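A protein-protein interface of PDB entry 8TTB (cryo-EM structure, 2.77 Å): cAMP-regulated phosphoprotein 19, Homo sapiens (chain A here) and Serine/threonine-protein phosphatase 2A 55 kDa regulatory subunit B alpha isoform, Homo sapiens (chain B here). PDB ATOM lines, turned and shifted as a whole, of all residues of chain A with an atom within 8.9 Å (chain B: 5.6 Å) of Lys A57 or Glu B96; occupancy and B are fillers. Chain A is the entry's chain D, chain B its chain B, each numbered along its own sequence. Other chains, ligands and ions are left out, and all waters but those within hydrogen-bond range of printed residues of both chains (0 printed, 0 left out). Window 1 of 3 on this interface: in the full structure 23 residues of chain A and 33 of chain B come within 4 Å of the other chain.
OE1 of Glu B96 lies within salt-bridge range of NZ of Lys A57, at 3.8 Å. The side-chain carboxylate of Glu B94 lies within hydrogen-bond range of the side-chain hydroxyl of Tyr A61 (2.6 Å).
Hydrophobic or aromatic side chains of chain A within 4 Å of the printed part of chain B: Tyr A61 and Pro A101.
The side-chain amide nitrogen (ND2) of Asn B118 is in hydrogen-bond range of the backbone carbonyl oxygen (O) of Glu B96 (3.1 Å). The side-chain amino group of Lys A60 sits at hydrogen-bond distance from the side-chain hydroxyl of Tyr A61.
Among the printed residues, merely in contact across the chains: Pro A101 with Pro B85 and Lys A57 with His B182.
Arg A52 touches none of the printed residues of chain B. Leu A55 touches none of the printed residues of chain B. Of chain B, only Glu B96 (3.8 Å) and His B182 (3.9 Å) come within 4 Å of Lys A57. Of the printed residues of chain B, Tyr A61 touches Glu B94. Of the printed residues of chain B, Pro A101 touches Pro B85. Of the printed residues of chain A, Pro B85 touches Pro A101. Of chain A, only Lys A57 (3.8 Å) comes within 4 Å of Glu B96. Of the printed residues of chain A, His B182 touches Lys A57 (3.9 Å). The nearest residue of chain B that does not touch Lys A57 is Leu B93 (4.9 Å). The nearest residue of chain A that does not touch Glu B96 is Gly A58 (7.0 Å).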
ATOM      1  N   LEU A  51       5.706 -40.547  12.040  1.00  0.00           N
ATOM      2  CA  LEU A  51       5.236 -39.192  12.307  1.00  0.00           C
ATOM      3  C   LEU A  51       6.336 -38.340  12.926  1.00  0.00           C
ATOM      4  O   LEU A  51       6.530 -37.182  12.540  1.00  0.00           O
ATOM      5  CB  LEU A  51       4.011 -39.232  13.219  1.00  0.00           C
ATOM      6  CG  LEU A  51       2.793 -39.970  12.664  1.00  0.00           C
ATOM      7  CD1 LEU A  51       1.696 -40.043  13.710  1.00  0.00           C
ATOM      8  CD2 LEU A  51       2.283 -39.297  11.401  1.00  0.00           C
ATOM      9  N   ARG A  52       7.069 -38.899  13.889  1.00  0.00           N
ATOM     10  CA  ARG A  52       8.083 -38.120  14.592  1.00  0.00           C
ATOM     11  C   ARG A  52       9.148 -37.608  13.632  1.00  0.00           C
ATOM     12  O   ARG A  52       9.570 -36.451  13.721  1.00  0.00           O
ATOM     13  CB  ARG A  52       8.718 -38.964  15.694  1.00  0.00           C
ATOM     14  CG  ARG A  52       7.732 -39.452  16.740  1.00  0.00           C
ATOM     15  CD  ARG A  52       8.331 -40.551  17.598  1.00  0.00           C
ATOM     16  NE  ARG A  52       9.397 -40.059  18.461  1.00  0.00           N
ATOM     17  CZ  ARG A  52      10.195 -40.839  19.179  1.00  0.00           C
ATOM     18  NH1 ARG A  52      10.101 -42.158  19.126  1.00  0.00           N
ATOM     19  NH2 ARG A  52      11.106 -40.282  19.969  1.00  0.00           N
ATOM     20  N   LYS A  53       9.599 -38.458  12.707  1.00  0.00           N
ATOM     21  CA  LYS A  53      10.619 -38.032  11.756  1.00  0.00           C
ATOM     22  C   LYS A  53      10.110 -36.898  10.876  1.00  0.00           C
ATOM     23  O   LYS A  53      10.877 -36.009  10.492  1.00  0.00           O
ATOM     24  CB  LYS A  53      11.073 -39.217  10.907  1.00  0.00           C
ATOM     25  CG  LYS A  53      11.842 -40.266  11.697  1.00  0.00           C
ATOM     26  CD  LYS A  53      12.256 -41.444  10.832  1.00  0.00           C
ATOM     27  CE  LYS A  53      13.071 -42.452  11.627  1.00  0.00           C
ATOM     28  NZ  LYS A  53      13.481 -43.622  10.803  1.00  0.00           N
ATOM     29  N   ARG A  54       8.817 -36.911  10.544  1.00  0.00           N
ATOM     30  CA  ARG A  54       8.262 -35.822   9.747  1.00  0.00           C
ATOM     31  C   ARG A  54       8.189 -34.532  10.554  1.00  0.00           C
ATOM     32  O   ARG A  54       8.340 -33.438   9.999  1.00  0.00           O
ATOM     33  CB  ARG A  54       6.885 -36.207   9.213  1.00  0.00           C
ATOM     34  CG  ARG A  54       6.927 -37.360   8.227  1.00  0.00           C
ATOM     35  CD  ARG A  54       5.647 -37.467   7.423  1.00  0.00           C
ATOM     36  NE  ARG A  54       5.472 -36.334   6.522  1.00  0.00           N
ATOM     37  CZ  ARG A  54       6.054 -36.221   5.335  1.00  0.00           C
ATOM     38  NH1 ARG A  54       6.873 -37.153   4.873  1.00  0.00           N
ATOM     39  NH2 ARG A  54       5.812 -35.144   4.593  1.00  0.00           N
ATOM     40  N   LEU A  55       7.960 -34.635  11.863  1.00  0.00           N
ATOM     41  CA  LEU A  55       8.001 -33.443  12.705  1.00  0.00           C
ATOM     42  C   LEU A  55       9.379 -32.799  12.667  1.00  0.00           C
ATOM     43  O   LEU A  55       9.499 -31.575  12.547  1.00  0.00           O
ATOM     44  CB  LEU A  55       7.626 -33.797  14.143  1.00  0.00           C
ATOM     45  CG  LEU A  55       6.224 -34.356  14.378  1.00  0.00           C
ATOM     46  CD1 LEU A  55       5.998 -34.583  15.860  1.00  0.00           C
ATOM     47  CD2 LEU A  55       5.164 -33.430  13.811  1.00  0.00           C
ATOM     48  N   GLN A  56      10.433 -33.610  12.768  1.00  0.00           N
ATOM     49  CA  GLN A  56      11.806 -33.112  12.769  1.00  0.00           C
ATOM     50  C   GLN A  56      12.296 -32.910  11.333  1.00  0.00           C
ATOM     51  O   GLN A  56      13.187 -33.596  10.837  1.00  0.00           O
ATOM     52  CB  GLN A  56      12.705 -34.074  13.532  1.00  0.00           C
ATOM     53  CG  GLN A  56      12.246 -34.361  14.951  1.00  0.00           C
ATOM     54  CD  GLN A  56      13.035 -35.479  15.601  1.00  0.00           C
ATOM     55  OE1 GLN A  56      13.664 -36.287  14.918  1.00  0.00           O
ATOM     56  NE2 GLN A  56      13.008 -35.530  16.928  1.00  0.00           N
ATOM     57  N   LYS A  57      11.674 -31.946  10.661  1.00  0.00           N
ATOM     58  CA  LYS A  57      12.049 -31.631   9.290  1.00  0.00           C
ATOM     59  C   LYS A  57      13.414 -30.955   9.259  1.00  0.00           C
ATOM     60  O   LYS A  57      13.685 -30.038  10.040  1.00  0.00           O
ATOM     61  CB  LYS A  57      10.995 -30.730   8.649  1.00  0.00           C
ATOM     62  CG  LYS A  57      11.211 -30.481   7.167  1.00  0.00           C
ATOM     63  CD  LYS A  57      10.102 -29.621   6.583  1.00  0.00           C
ATOM     64  CE  LYS A  57      10.261 -29.449   5.081  1.00  0.00           C
ATOM     65  NZ  LYS A  57       9.190 -28.596   4.495  1.00  0.00           N
ATOM     66  N   GLY A  58      14.273 -31.411   8.352  1.00  0.00           N
ATOM     67  CA  GLY A  58      15.587 -30.823   8.184  1.00  0.00           C
ATOM     68  C   GLY A  58      16.625 -31.358   9.149  1.00  0.00           C
ATOM     69  O   GLY A  58      17.467 -32.175   8.764  1.00  0.00           O
ATOM     70  N   GLN A  59      16.577 -30.911  10.405  1.00  0.00           N
ATOM     71  CA  GLN A  59      17.566 -31.312  11.407  1.00  0.00           C
ATOM     72  C   GLN A  59      18.980 -31.053  10.899  1.00  0.00           C
ATOM     73  O   GLN A  59      19.905 -31.828  11.143  1.00  0.00           O
ATOM     74  CB  GLN A  59      17.399 -32.783  11.788  1.00  0.00           C
ATOM     75  CG  GLN A  59      15.999 -33.170  12.217  1.00  0.00           C
ATOM     76  CD  GLN A  59      15.866 -34.656  12.481  1.00  0.00           C
ATOM     77  OE1 GLN A  59      14.934 -35.302  12.002  1.00  0.00           O
ATOM     78  NE2 GLN A  59      16.799 -35.208  13.249  1.00  0.00           N
ATOM     79  N   LYS A  60      19.146 -29.948  10.173  1.00  0.00           N
ATOM     80  CA  LYS A  60      20.404 -29.716   9.472  1.00  0.00           C
ATOM     81  C   LYS A  60      21.558 -29.500  10.442  1.00  0.00           C
ATOM     82  O   LYS A  60      22.652 -30.038  10.237  1.00  0.00           O
ATOM     83  CB  LYS A  60      20.260 -28.520   8.533  1.00  0.00           C
ATOM     84  CG  LYS A  60      21.466 -28.291   7.641  1.00  0.00           C
ATOM     85  CD  LYS A  60      21.208 -27.184   6.636  1.00  0.00           C
ATOM     86  CE  LYS A  60      22.427 -26.927   5.767  1.00  0.00           C
ATOM     87  NZ  LYS A  60      22.199 -25.816   4.804  1.00  0.00           N
ATOM     88  N   TYR A  61      21.340 -28.730  11.504  1.00  0.00           N
ATOM     89  CA  TYR A  61      22.422 -28.249  12.348  1.00  0.00           C
ATOM     90  C   TYR A  61      22.381 -28.891  13.728  1.00  0.00           C
ATOM     91  O   TYR A  61      21.312 -29.172  14.276  1.00  0.00           O
ATOM     92  CB  TYR A  61      22.362 -26.727  12.491  1.00  0.00           C
ATOM     93  CG  TYR A  61      22.477 -26.008  11.172  1.00  0.00           C
ATOM     94  CD1 TYR A  61      23.694 -25.924  10.512  1.00  0.00           C
ATOM     95  CD2 TYR A  61      21.372 -25.417  10.583  1.00  0.00           C
ATOM     96  CE1 TYR A  61      23.805 -25.271   9.305  1.00  0.00           C
ATOM     97  CE2 TYR A  61      21.473 -24.762   9.376  1.00  0.00           C
ATOM     98  CZ  TYR A  61      22.692 -24.692   8.741  1.00  0.00           C
ATOM     99  OH  TYR A  61      22.799 -24.039   7.536  1.00  0.00           O
ATOM    100  N   PRO A 101      21.030 -17.290   6.424  1.00  0.00           N
ATOM    101  CA  PRO A 101      20.505 -16.371   5.411  1.00  0.00           C
ATOM    102  C   PRO A 101      21.263 -15.053   5.405  1.00  0.00           C
ATOM    103  O   PRO A 101      21.973 -14.704   6.351  1.00  0.00           O
ATOM    104  CB  PRO A 101      19.045 -16.172   5.833  1.00  0.00           C
ATOM    105  CG  PRO A 101      18.711 -17.388   6.618  1.00  0.00           C
ATOM    106  CD  PRO A 101      19.972 -17.777   7.326  1.00  0.00           C
ATOM    107  N   GLU B  84      10.650 -13.713   5.401  1.00  0.00           N
ATOM    108  CA  GLU B  84      12.031 -13.830   4.966  1.00  0.00           C
ATOM    109  C   GLU B  84      12.693 -14.982   5.702  1.00  0.00           C
ATOM    110  O   GLU B  84      12.279 -15.332   6.811  1.00  0.00           O
ATOM    111  CB  GLU B  84      12.809 -12.536   5.237  1.00  0.00           C
ATOM    112  CG  GLU B  84      12.194 -11.300   4.606  1.00  0.00           C
ATOM    113  CD  GLU B  84      12.888 -10.023   5.031  1.00  0.00           C
ATOM    114  OE1 GLU B  84      13.807 -10.097   5.872  1.00  0.00           O
ATOM    115  OE2 GLU B  84      12.513  -8.944   4.524  1.00  0.00           O
ATOM    116  N   PRO B  85      13.720 -15.594   5.114  1.00  0.00           N
ATOM    117  CA  PRO B  85      14.402 -16.690   5.808  1.00  0.00           C
ATOM    118  C   PRO B  85      14.956 -16.225   7.145  1.00  0.00           C
ATOM    119  O   PRO B  85      15.456 -15.108   7.277  1.00  0.00           O
ATOM    120  CB  PRO B  85      15.521 -17.086   4.839  1.00  0.00           C
ATOM    121  CG  PRO B  85      15.074 -16.597   3.514  1.00  0.00           C
ATOM    122  CD  PRO B  85      14.289 -15.353   3.778  1.00  0.00           C
ATOM    123  N   GLU B  86      14.857 -17.098   8.143  1.00  0.00           N
ATOM    124  CA  GLU B  86      15.315 -16.784   9.487  1.00  0.00           C
ATOM    125  C   GLU B  86      15.987 -18.007  10.086  1.00  0.00           C
ATOM    126  O   GLU B  86      15.751 -19.142   9.670  1.00  0.00           O
ATOM    127  CB  GLU B  86      14.163 -16.330  10.391  1.00  0.00           C
ATOM    128  CG  GLU B  86      13.540 -15.009   9.984  1.00  0.00           C
ATOM    129  CD  GLU B  86      12.465 -14.553  10.950  1.00  0.00           C
ATOM    130  OE1 GLU B  86      12.185 -15.291  11.918  1.00  0.00           O
ATOM    131  OE2 GLU B  86      11.901 -13.459  10.742  1.00  0.00           O
ATOM    132  N   LEU B  93      17.569 -24.002  14.122  1.00  0.00           N
ATOM    133  CA  LEU B  93      16.719 -24.375  13.003  1.00  0.00           C
ATOM    134  C   LEU B  93      16.585 -23.201  12.045  1.00  0.00           C
ATOM    135  O   LEU B  93      16.484 -22.048  12.472  1.00  0.00           O
ATOM    136  CB  LEU B  93      15.330 -24.805  13.481  1.00  0.00           C
ATOM    137  CG  LEU B  93      15.259 -26.085  14.313  1.00  0.00           C
ATOM    138  CD1 LEU B  93      13.846 -26.304  14.822  1.00  0.00           C
ATOM    139  CD2 LEU B  93      15.726 -27.282  13.502  1.00  0.00           C
ATOM    140  N   GLU B  94      16.586 -23.502  10.751  1.00  0.00           N
ATOM    141  CA  GLU B  94      16.323 -22.507   9.721  1.00  0.00           C
ATOM    142  C   GLU B  94      14.824 -22.464   9.453  1.00  0.00           C
ATOM    143  O   GLU B  94      14.246 -23.449   8.982  1.00  0.00           O
ATOM    144  CB  GLU B  94      17.090 -22.830   8.440  1.00  0.00           C
ATOM    145  CG  GLU B  94      18.596 -22.730   8.578  1.00  0.00           C
ATOM    146  CD  GLU B  94      19.318 -23.011   7.276  1.00  0.00           C
ATOM    147  OE1 GLU B  94      18.649 -23.397   6.295  1.00  0.00           O
ATOM    148  OE2 GLU B  94      20.556 -22.844   7.231  1.00  0.00           O
ATOM    149  N   ILE B  95      14.200 -21.331   9.756  1.00  0.00           N
ATOM    150  CA  ILE B  95      12.765 -21.164   9.551  1.00  0.00           C
ATOM    151  C   ILE B  95      12.538 -20.835   8.080  1.00  0.00           C
ATOM    152  O   ILE B  95      12.914 -19.760   7.608  1.00  0.00           O
ATOM    153  CB  ILE B  95      12.191 -20.070  10.458  1.00  0.00           C
ATOM    154  CG1 ILE B  95      12.513 -20.369  11.923  1.00  0.00           C
ATOM    155  CG2 ILE B  95      10.684 -19.954  10.260  1.00  0.00           C
ATOM    156  CD1 ILE B  95      12.027 -19.303  12.884  1.00  0.00           C
ATOM    157  N   GLU B  96      11.922 -21.763   7.352  1.00  0.00           N
ATOM    158  CA  GLU B  96      11.607 -21.514   5.954  1.00  0.00           C
ATOM    159  C   GLU B  96      10.614 -20.364   5.834  1.00  0.00           C
ATOM    160  O   GLU B  96       9.726 -20.199   6.673  1.00  0.00           O
ATOM    161  CB  GLU B  96      11.036 -22.774   5.305  1.00  0.00           C
ATOM    162  CG  GLU B  96      12.025 -23.918   5.215  1.00  0.00           C
ATOM    163  CD  GLU B  96      11.474 -25.106   4.452  1.00  0.00           C
ATOM    164  OE1 GLU B  96      10.318 -25.030   3.985  1.00  0.00           O
ATOM    165  OE2 GLU B  96      12.197 -26.115   4.317  1.00  0.00           O
ATOM    166  N   GLU B  97      10.772 -19.571   4.780  1.00  0.00           N
ATOM    167  CA  GLU B  97       9.913 -18.424   4.525  1.00  0.00           C
ATOM    168  C   GLU B  97       8.687 -18.784   3.696  1.00  0.00           C
ATOM    169  O   GLU B  97       7.923 -17.889   3.325  1.00  0.00           O
ATOM    170  CB  GLU B  97      10.706 -17.311   3.829  1.00  0.00           C
ATOM    171  CG  GLU B  97      11.105 -17.591   2.381  1.00  0.00           C
ATOM    172  CD  GLU B  97      12.240 -18.587   2.258  1.00  0.00           C
ATOM    173  OE1 GLU B  97      12.674 -19.125   3.297  1.00  0.00           O
ATOM    174  OE2 GLU B  97      12.698 -18.831   1.124  1.00  0.00           O
ATOM    175  N   LYS B  98       8.485 -20.065   3.400  1.00  0.00           N
ATOM    176  CA  LYS B  98       7.342 -20.481   2.601  1.00  0.00           C
ATOM    177  C   LYS B  98       6.045 -19.999   3.234  1.00  0.00           C
ATOM    178  O   LYS B  98       5.859 -20.076   4.451  1.00  0.00           O
ATOM    179  CB  LYS B  98       7.326 -22.004   2.465  1.00  0.00           C
ATOM    180  CG  LYS B  98       6.056 -22.570   1.851  1.00  0.00           C
ATOM    181  CD  LYS B  98       6.127 -24.080   1.736  1.00  0.00           C
ATOM    182  CE  LYS B  98       4.858 -24.648   1.125  1.00  0.00           C
ATOM    183  NZ  LYS B  98       4.901 -26.132   1.022  1.00  0.00           N
ATOM    184  N   ASN B 118       3.927 -18.397   7.771  1.00  0.00           N
ATOM    185  CA  ASN B 118       4.898 -19.432   7.463  1.00  0.00           C
ATOM    186  C   ASN B 118       4.791 -20.513   8.536  1.00  0.00           C
ATOM    187  O   ASN B 118       3.835 -20.552   9.313  1.00  0.00           O
ATOM    188  CB  ASN B 118       6.302 -18.843   7.361  1.00  0.00           C
ATOM    189  CG  ASN B 118       6.878 -18.468   8.705  1.00  0.00           C
ATOM    190  OD1 ASN B 118       6.145 -18.151   9.639  1.00  0.00           O
ATOM    191  ND2 ASN B 118       8.198 -18.498   8.811  1.00  0.00           N
ATOM    192  N   ASP B 119       5.772 -21.413   8.591  1.00  0.00           N
ATOM    193  CA  ASP B 119       5.710 -22.511   9.547  1.00  0.00           C
ATOM    194  C   ASP B 119       5.696 -22.034  10.993  1.00  0.00           C
ATOM    195  O   ASP B 119       5.278 -22.792  11.873  1.00  0.00           O
ATOM    196  CB  ASP B 119       6.890 -23.458   9.332  1.00  0.00           C
ATOM    197  CG  ASP B 119       6.708 -24.350   8.122  1.00  0.00           C
ATOM    198  OD1 ASP B 119       5.565 -24.785   7.870  1.00  0.00           O
ATOM    199  OD2 ASP B 119       7.706 -24.616   7.422  1.00  0.00           O
ATOM    200  N   HIS B 182       5.353 -26.904  13.295  1.00  0.00           N
ATOM    201  CA  HIS B 182       5.081 -26.134  12.088  1.00  0.00           C
ATOM    202  C   HIS B 182       3.593 -25.830  11.976  1.00  0.00           C
ATOM    203  O   HIS B 182       2.762 -26.742  12.011  1.00  0.00           O
ATOM    204  CB  HIS B 182       5.562 -26.898  10.858  1.00  0.00           C
ATOM    205  CG  HIS B 182       7.046 -27.071  10.803  1.00  0.00           C
ATOM    206  ND1 HIS B 182       7.685 -27.690   9.751  1.00  0.00           N
ATOM    207  CD2 HIS B 182       8.018 -26.703  11.671  1.00  0.00           C
ATOM    208  CE1 HIS B 182       8.987 -27.696   9.974  1.00  0.00           C
ATOM    209  NE2 HIS B 182       9.215 -27.103  11.132  1.00  0.00           N
